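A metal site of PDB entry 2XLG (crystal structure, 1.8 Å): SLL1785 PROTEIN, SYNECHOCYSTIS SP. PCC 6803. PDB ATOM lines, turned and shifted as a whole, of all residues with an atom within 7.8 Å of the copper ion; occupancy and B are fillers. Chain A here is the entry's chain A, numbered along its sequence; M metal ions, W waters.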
ATOM      1  N   PRO A  56     -24.798  -7.096 -13.917  1.00  0.00           N
ATOM      2  CA  PRO A  56     -23.959  -6.565 -12.854  1.00  0.00           C
ATOM      3  C   PRO A  56     -24.547  -6.698 -11.473  1.00  0.00           C
ATOM      4  O   PRO A  56     -25.746  -6.435 -11.269  1.00  0.00           O
ATOM      5  CB  PRO A  56     -23.806  -5.081 -13.227  1.00  0.00           C
ATOM      6  CG  PRO A  56     -25.049  -4.760 -14.001  1.00  0.00           C
ATOM      7  CD  PRO A  56     -25.427  -6.026 -14.700  1.00  0.00           C
ATOM      8  N   MET A  57     -23.685  -7.062 -10.524  1.00  0.00           N
ATOM      9  CA  MET A  57     -24.142  -7.090  -9.157  1.00  0.00           C
ATOM     10  C   MET A  57     -24.379  -5.665  -8.679  1.00  0.00           C
ATOM     11  O   MET A  57     -24.000  -4.705  -9.354  1.00  0.00           O
ATOM     12  CB  MET A  57     -23.112  -7.806  -8.282  1.00  0.00           C
ATOM     13  CG  MET A  57     -23.175  -9.294  -8.425  1.00  0.00           C
ATOM     14  SD  MET A  57     -21.655  -9.947  -7.783  1.00  0.00           S
ATOM     15  CE  MET A  57     -21.731 -11.676  -8.321  1.00  0.00           C
ATOM     16  N   PRO A  58     -25.066  -5.521  -7.549  1.00  0.00           N
ATOM     17  CA  PRO A  58     -25.354  -4.164  -7.067  1.00  0.00           C
ATOM     18  C   PRO A  58     -24.163  -3.232  -6.977  1.00  0.00           C
ATOM     19  O   PRO A  58     -23.075  -3.613  -6.483  1.00  0.00           O
ATOM     20  CB  PRO A  58     -25.998  -4.413  -5.725  1.00  0.00           C
ATOM     21  CG  PRO A  58     -26.634  -5.721  -5.873  1.00  0.00           C
ATOM     22  CD  PRO A  58     -25.702  -6.529  -6.689  1.00  0.00           C
ATOM     23  N   HIS A  59     -24.395  -2.018  -7.474  1.00  0.00           N
ATOM     24  CA  HIS A  59     -23.389  -0.984  -7.510  1.00  0.00           C
ATOM     25  C   HIS A  59     -24.041   0.403  -7.490  1.00  0.00           C
ATOM     26  O   HIS A  59     -25.250   0.537  -7.715  1.00  0.00           O
ATOM     27  CB  HIS A  59     -22.492  -1.155  -8.722  1.00  0.00           C
ATOM     28  CG  HIS A  59     -23.179  -1.035 -10.054  1.00  0.00           C
ATOM     29  ND1 HIS A  59     -23.884  -2.082 -10.628  1.00  0.00           N
ATOM     30  CD2 HIS A  59     -23.279   0.005 -10.910  1.00  0.00           C
ATOM     31  CE1 HIS A  59     -24.358  -1.685 -11.800  1.00  0.00           C
ATOM     32  NE2 HIS A  59     -24.013  -0.415 -11.996  1.00  0.00           N
ATOM     33  N   ILE A  60     -23.212   1.400  -7.247  1.00  0.00           N
ATOM     34  CA  ILE A  60     -23.623   2.785  -7.097  1.00  0.00           C
ATOM     35  C   ILE A  60     -22.643   3.644  -7.884  1.00  0.00           C
ATOM     36  O   ILE A  60     -21.419   3.471  -7.736  1.00  0.00           O
ATOM     37  CB  ILE A  60     -23.593   3.246  -5.625  1.00  0.00           C
ATOM     38  CG1 ILE A  60     -24.475   2.376  -4.720  1.00  0.00           C
ATOM     39  CG2 ILE A  60     -23.961   4.737  -5.519  1.00  0.00           C
ATOM     40  CD1 ILE A  60     -24.060   2.411  -3.225  1.00  0.00           C
ATOM     41  N   HIS A  61     -23.169   4.557  -8.714  1.00  0.00           N
ATOM     42  CA  HIS A  61     -22.375   5.495  -9.502  1.00  0.00           C
ATOM     43  C   HIS A  61     -22.296   6.888  -8.866  1.00  0.00           C
ATOM     44  O   HIS A  61     -23.269   7.387  -8.271  1.00  0.00           O
ATOM     45  CB  HIS A  61     -22.936   5.704 -10.891  1.00  0.00           C
ATOM     46  CG  HIS A  61     -23.002   4.478 -11.713  1.00  0.00           C
ATOM     47  ND1 HIS A  61     -22.031   4.141 -12.626  1.00  0.00           N
ATOM     48  CD2 HIS A  61     -23.950   3.512 -11.799  1.00  0.00           C
ATOM     49  CE1 HIS A  61     -22.369   3.007 -13.218  1.00  0.00           C
ATOM     50  NE2 HIS A  61     -23.510   2.598 -12.724  1.00  0.00           N
ATOM     51  N   ILE A  64     -21.775   9.418 -13.157  1.00  0.00           N
ATOM     52  CA  ILE A  64     -22.708   9.331 -14.277  1.00  0.00           C
ATOM     53  C   ILE A  64     -24.106   9.102 -13.766  1.00  0.00           C
ATOM     54  O   ILE A  64     -24.292   8.654 -12.632  1.00  0.00           O
ATOM     55  CB  ILE A  64     -22.356   8.204 -15.316  1.00  0.00           C
ATOM     56  CG1 ILE A  64     -22.420   6.795 -14.705  1.00  0.00           C
ATOM     57  CG2 ILE A  64     -20.948   8.440 -15.901  1.00  0.00           C
ATOM     58  CD1 ILE A  64     -23.819   6.079 -14.849  1.00  0.00           C
ATOM     59  N   ASN A  65     -25.052   9.433 -14.623  1.00  0.00           N
ATOM     60  CA  ASN A  65     -26.456   9.040 -14.486  1.00  0.00           C
ATOM     61  C   ASN A  65     -26.693   7.967 -15.556  1.00  0.00           C
ATOM     62  O   ASN A  65     -26.130   8.037 -16.650  1.00  0.00           O
ATOM     63  CB  ASN A  65     -27.381  10.243 -14.695  1.00  0.00           C
ATOM     64  CG  ASN A  65     -27.284  11.272 -13.584  1.00  0.00           C
ATOM     65  OD1 ASN A  65     -27.554  10.970 -12.425  1.00  0.00           O
ATOM     66  ND2 ASN A  65     -26.887  12.478 -13.946  1.00  0.00           N
ATOM     67  N   GLU A  66     -27.505   6.966 -15.260  1.00  0.00           N
ATOM     68  CA  GLU A  66     -27.603   5.805 -16.144  1.00  0.00           C
ATOM     69  C   GLU A  66     -29.022   5.548 -16.637  1.00  0.00           C
ATOM     70  O   GLU A  66     -29.969   5.764 -15.899  1.00  0.00           O
ATOM     71  CB  GLU A  66     -27.076   4.553 -15.434  1.00  0.00           C
ATOM     72  CG  GLU A  66     -27.068   3.266 -16.298  1.00  0.00           C
ATOM     73  CD  GLU A  66     -26.111   2.204 -15.740  1.00  0.00           C
ATOM     74  OE1 GLU A  66     -25.896   2.183 -14.524  1.00  0.00           O
ATOM     75  OE2 GLU A  66     -25.574   1.380 -16.512  1.00  0.00           O
ATOM     76  N   TRP A  67     -29.151   5.042 -17.860  1.00  0.00           N
ATOM     77  CA  TRP A  67     -30.424   4.535 -18.367  1.00  0.00           C
ATOM     78  C   TRP A  67     -30.271   3.090 -18.742  1.00  0.00           C
ATOM     79  O   TRP A  67     -29.218   2.694 -19.266  1.00  0.00           O
ATOM     80  CB  TRP A  67     -30.861   5.276 -19.635  1.00  0.00           C
ATOM     81  CG  TRP A  67     -31.264   6.698 -19.499  1.00  0.00           C
ATOM     82  CD1 TRP A  67     -32.553   7.182 -19.620  1.00  0.00           C
ATOM     83  CD2 TRP A  67     -30.433   7.838 -19.291  1.00  0.00           C
ATOM     84  NE1 TRP A  67     -32.550   8.539 -19.491  1.00  0.00           N
ATOM     85  CE2 TRP A  67     -31.268   8.973 -19.287  1.00  0.00           C
ATOM     86  CE3 TRP A  67     -29.052   8.007 -19.087  1.00  0.00           C
ATOM     87  CZ2 TRP A  67     -30.775  10.259 -19.096  1.00  0.00           C
ATOM     88  CZ3 TRP A  67     -28.564   9.293 -18.905  1.00  0.00           C
ATOM     89  CH2 TRP A  67     -29.426  10.403 -18.909  1.00  0.00           C
ATOM     90  N   PHE A  68     -31.316   2.303 -18.499  1.00  0.00           N
ATOM     91  CA  PHE A  68     -31.383   0.922 -18.969  1.00  0.00           C
ATOM     92  C   PHE A  68     -32.583   0.812 -19.899  1.00  0.00           C
ATOM     93  O   PHE A  68     -33.676   1.345 -19.590  1.00  0.00           O
ATOM     94  CB  PHE A  68     -31.566  -0.064 -17.810  1.00  0.00           C
ATOM     95  CG  PHE A  68     -30.547   0.046 -16.702  1.00  0.00           C
ATOM     96  CD1 PHE A  68     -29.346  -0.632 -16.775  1.00  0.00           C
ATOM     97  CD2 PHE A  68     -30.799   0.816 -15.574  1.00  0.00           C
ATOM     98  CE1 PHE A  68     -28.412  -0.552 -15.757  1.00  0.00           C
ATOM     99  CE2 PHE A  68     -29.858   0.874 -14.549  1.00  0.00           C
ATOM    100  CZ  PHE A  68     -28.669   0.206 -14.650  1.00  0.00           C
ATOM    101  N   SER A 114     -31.858   5.703 -13.920  1.00  0.00           N
ATOM    102  CA  SER A 114     -31.286   5.589 -12.581  1.00  0.00           C
ATOM    103  C   SER A 114     -30.225   6.651 -12.339  1.00  0.00           C
ATOM    104  O   SER A 114     -29.092   6.535 -12.813  1.00  0.00           O
ATOM    105  CB  SER A 114     -30.701   4.188 -12.360  1.00  0.00           C
ATOM    106  OG  SER A 114     -30.306   3.973 -11.005  1.00  0.00           O
ATOM    107  N   TYR A 118     -28.007   6.116  -6.548  1.00  0.00           N
ATOM    108  CA  TYR A 118     -28.896   4.981  -6.315  1.00  0.00           C
ATOM    109  C   TYR A 118     -28.083   3.720  -6.422  1.00  0.00           C
ATOM    110  O   TYR A 118     -27.163   3.656  -7.189  1.00  0.00           O
ATOM    111  CB  TYR A 118     -30.066   4.982  -7.294  1.00  0.00           C
ATOM    112  CG  TYR A 118     -31.123   6.007  -6.953  1.00  0.00           C
ATOM    113  CD1 TYR A 118     -32.057   5.752  -5.955  1.00  0.00           C
ATOM    114  CD2 TYR A 118     -31.216   7.208  -7.651  1.00  0.00           C
ATOM    115  CE1 TYR A 118     -33.029   6.706  -5.628  1.00  0.00           C
ATOM    116  CE2 TYR A 118     -32.198   8.163  -7.342  1.00  0.00           C
ATOM    117  CZ  TYR A 118     -33.090   7.906  -6.332  1.00  0.00           C
ATOM    118  OH  TYR A 118     -34.043   8.832  -6.016  1.00  0.00           O
ATOM    119  N   MET A 119     -28.454   2.710  -5.650  1.00  0.00           N
ATOM    120  CA  MET A 119     -27.898   1.385  -5.800  1.00  0.00           C
ATOM    121  C   MET A 119     -28.755   0.629  -6.777  1.00  0.00           C
ATOM    122  O   MET A 119     -29.987   0.615  -6.649  1.00  0.00           O
ATOM    123  CB  MET A 119     -27.810   0.649  -4.466  1.00  0.00           C
ATOM    124  CG  MET A 119     -27.081  -0.715  -4.517  1.00  0.00           C
ATOM    125  SD  MET A 119     -27.263  -1.629  -2.969  1.00  0.00           S
ATOM    126  CE  MET A 119     -26.530  -0.522  -1.772  1.00  0.00           C
ATOM    127  N   HIS A 120     -28.111  -0.027  -7.741  1.00  0.00           N
ATOM    128  CA  HIS A 120     -28.843  -0.785  -8.752  1.00  0.00           C
ATOM    129  C   HIS A 120     -28.006  -1.945  -9.304  1.00  0.00           C
ATOM    130  O   HIS A 120     -26.808  -2.088  -9.027  1.00  0.00           O
ATOM    131  CB  HIS A 120     -29.349   0.147  -9.889  1.00  0.00           C
ATOM    132  CG  HIS A 120     -28.265   0.775 -10.714  1.00  0.00           C
ATOM    133  ND1 HIS A 120     -28.350   2.064 -11.176  1.00  0.00           N
ATOM    134  CD2 HIS A 120     -27.057   0.315 -11.130  1.00  0.00           C
ATOM    135  CE1 HIS A 120     -27.248   2.373 -11.844  1.00  0.00           C
ATOM    136  NE2 HIS A 120     -26.454   1.327 -11.835  1.00  0.00           N
ATOM    137  N   GLY A 121     -28.676  -2.800 -10.066  1.00  0.00           N
ATOM    138  CA  GLY A 121     -28.057  -3.886 -10.783  1.00  0.00           C
ATOM    139  C   GLY A 121     -29.095  -4.536 -11.659  1.00  0.00           C
ATOM    140  O   GLY A 121     -30.260  -4.109 -11.689  1.00  0.00           O
ATOM    141  N   PHE A 122     -28.699  -5.570 -12.356  1.00  0.00           N
ATOM    142  CA  PHE A 122     -29.678  -6.323 -13.095  1.00  0.00           C
ATOM    143  C   PHE A 122     -29.184  -7.735 -13.314  1.00  0.00           C
ATOM    144  O   PHE A 122     -28.002  -8.039 -13.212  1.00  0.00           O
ATOM    145  CB  PHE A 122     -30.127  -5.617 -14.402  1.00  0.00           C
ATOM    146  CG  PHE A 122     -29.074  -5.516 -15.467  1.00  0.00           C
ATOM    147  CD1 PHE A 122     -28.387  -4.322 -15.669  1.00  0.00           C
ATOM    148  CD2 PHE A 122     -28.827  -6.581 -16.323  1.00  0.00           C
ATOM    149  CE1 PHE A 122     -27.459  -4.203 -16.666  1.00  0.00           C
ATOM    150  CE2 PHE A 122     -27.880  -6.477 -17.318  1.00  0.00           C
ATOM    151  CZ  PHE A 122     -27.177  -5.294 -17.484  1.00  0.00           C
ATOM    152  N   PHE A 134     -27.465  -0.045 -22.095  1.00  0.00           N
ATOM    153  CA  PHE A 134     -27.320   0.901 -21.011  1.00  0.00           C
ATOM    154  C   PHE A 134     -26.435   2.049 -21.436  1.00  0.00           C
ATOM    155  O   PHE A 134     -25.507   1.880 -22.243  1.00  0.00           O
ATOM    156  CB  PHE A 134     -26.861   0.226 -19.686  1.00  0.00           C
ATOM    157  CG  PHE A 134     -25.553  -0.584 -19.774  1.00  0.00           C
ATOM    158  CD1 PHE A 134     -24.336   0.025 -19.532  1.00  0.00           C
ATOM    159  CD2 PHE A 134     -25.579  -1.950 -20.004  1.00  0.00           C
ATOM    160  CE1 PHE A 134     -23.139  -0.709 -19.569  1.00  0.00           C
ATOM    161  CE2 PHE A 134     -24.387  -2.684 -20.050  1.00  0.00           C
ATOM    162  CZ  PHE A 134     -23.162  -2.050 -19.835  1.00  0.00           C
ATOM    163  N   VAL A 135     -26.747   3.210 -20.898  1.00  0.00           N
ATOM    164  CA  VAL A 135     -26.196   4.473 -21.332  1.00  0.00           C
ATOM    165  C   VAL A 135     -25.740   5.177 -20.079  1.00  0.00           C
ATOM    166  O   VAL A 135     -26.482   5.259 -19.113  1.00  0.00           O
ATOM    167  CB  VAL A 135     -27.267   5.319 -22.069  1.00  0.00           C
ATOM    168  CG1 VAL A 135     -26.686   6.622 -22.588  1.00  0.00           C
ATOM    169  CG2 VAL A 135     -27.873   4.520 -23.218  1.00  0.00           C
ATOM    170  N   TRP A 136     -24.499   5.640 -20.103  1.00  0.00           N
ATOM    171  CA  TRP A 136     -23.942   6.434 -19.018  1.00  0.00           C
ATOM    172  C   TRP A 136     -23.732   7.857 -19.526  1.00  0.00           C
ATOM    173  O   TRP A 136     -22.966   8.068 -20.467  1.00  0.00           O
ATOM    174  CB  TRP A 136     -22.566   5.886 -18.604  1.00  0.00           C
ATOM    175  CG  TRP A 136     -22.535   4.537 -17.954  1.00  0.00           C
ATOM    176  CD1 TRP A 136     -23.557   3.652 -17.816  1.00  0.00           C
ATOM    177  CD2 TRP A 136     -21.371   3.892 -17.436  1.00  0.00           C
ATOM    178  NE1 TRP A 136     -23.109   2.506 -17.197  1.00  0.00           N
ATOM    179  CE2 TRP A 136     -21.766   2.629 -16.962  1.00  0.00           C
ATOM    180  CE3 TRP A 136     -20.031   4.274 -17.310  1.00  0.00           C
ATOM    181  CZ2 TRP A 136     -20.883   1.746 -16.362  1.00  0.00           C
ATOM    182  CZ3 TRP A 136     -19.145   3.387 -16.723  1.00  0.00           C
ATOM    183  CH2 TRP A 136     -19.573   2.153 -16.264  1.00  0.00           C
ATOM    184  N   TYR A 155     -13.053   1.196 -18.043  1.00  0.00           N
ATOM    185  CA  TYR A 155     -13.525   0.339 -16.975  1.00  0.00           C
ATOM    186  C   TYR A 155     -13.701  -1.102 -17.443  1.00  0.00           C
ATOM    187  O   TYR A 155     -13.124  -2.032 -16.881  1.00  0.00           O
ATOM    188  CB  TYR A 155     -14.837   0.877 -16.409  1.00  0.00           C
ATOM    189  CG  TYR A 155     -15.493  -0.011 -15.366  1.00  0.00           C
ATOM    190  CD1 TYR A 155     -14.737  -0.594 -14.339  1.00  0.00           C
ATOM    191  CD2 TYR A 155     -16.856  -0.278 -15.421  1.00  0.00           C
ATOM    192  CE1 TYR A 155     -15.340  -1.384 -13.380  1.00  0.00           C
ATOM    193  CE2 TYR A 155     -17.458  -1.082 -14.474  1.00  0.00           C
ATOM    194  CZ  TYR A 155     -16.707  -1.633 -13.456  1.00  0.00           C
ATOM    195  OH  TYR A 155     -17.309  -2.436 -12.509  1.00  0.00           O
ATOM    196  N   ILE A 189     -17.337   4.313  -9.059  1.00  0.00           N
ATOM    197  CA  ILE A 189     -18.327   3.259  -8.849  1.00  0.00           C
ATOM    198  C   ILE A 189     -17.970   2.431  -7.619  1.00  0.00           C
ATOM    199  O   ILE A 189     -16.848   1.967  -7.508  1.00  0.00           O
ATOM    200  CB  ILE A 189     -18.446   2.313 -10.084  1.00  0.00           C
ATOM    201  CG1 ILE A 189     -18.871   3.120 -11.312  1.00  0.00           C
ATOM    202  CG2 ILE A 189     -19.520   1.213  -9.795  1.00  0.00           C
ATOM    203  CD1 ILE A 189     -18.621   2.451 -12.609  1.00  0.00           C
ATOM    204  N   GLN A 191     -18.702  -0.969  -6.450  1.00  0.00           N
ATOM    205  CA  GLN A 191     -19.173  -2.211  -7.051  1.00  0.00           C
ATOM    206  C   GLN A 191     -19.037  -3.394  -6.092  1.00  0.00           C
ATOM    207  O   GLN A 191     -17.946  -3.706  -5.621  1.00  0.00           O
ATOM    208  CB  GLN A 191     -18.409  -2.458  -8.339  1.00  0.00           C
ATOM    209  CG  GLN A 191     -18.767  -3.766  -9.060  1.00  0.00           C
ATOM    210  CD  GLN A 191     -20.223  -3.778  -9.494  1.00  0.00           C
ATOM    211  OE1 GLN A 191     -20.629  -2.991 -10.345  1.00  0.00           O
ATOM    212  NE2 GLN A 191     -21.022  -4.650  -8.897  1.00  0.00           N
HETATM  213 CU    CU M   1     -24.832   1.021 -13.194  1.00  0.00          CU
HETATM  214  O   HOH W   1     -24.796  -0.390 -14.770  1.00  0.00           O
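The copper ion is bound by a ring nitrogen (NE2) of His 59 (2.0 Å), the side-chain carboxylate (OE1) of Glu 66 (2.1 Å), a ring nitrogen (NE2) of His 61 (2.1 Å), water W1 (2.1 Å) and a ring nitrogen (NE2) of His 120 (2.1 Å).
The copper ion has five donor atoms within binding distance.
Four residues have an atom within 4 Å of the copper ion: His 59, His 61, Glu 66 and His 120.
The nearest printed residue that does not touch the copper ion is Phe 68 (4.2 Å).
ND1 of His 59 lies close to OE1 of Gln 191 (3.4 Å).
A ring nitrogen (ND1) of His 59 lies within hydrogen-bond range of the backbone carbonyl oxygen of Met 57, at 2.9 Å.
The side-chain carboxylate of Glu 66 is in hydrogen-bond range of the indole nitrogen of Trp 136 (2.8 Å).
The backbone carbonyl oxygen (O) of Glu 66 sits at hydrogen-bond distance from the backbone NH (N) of Ser 114, 2.7 Å away.
A ring nitrogen (ND1) of His 120 lies within hydrogen-bond range of the side-chain hydroxyl of Ser 114 (2.7 Å).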
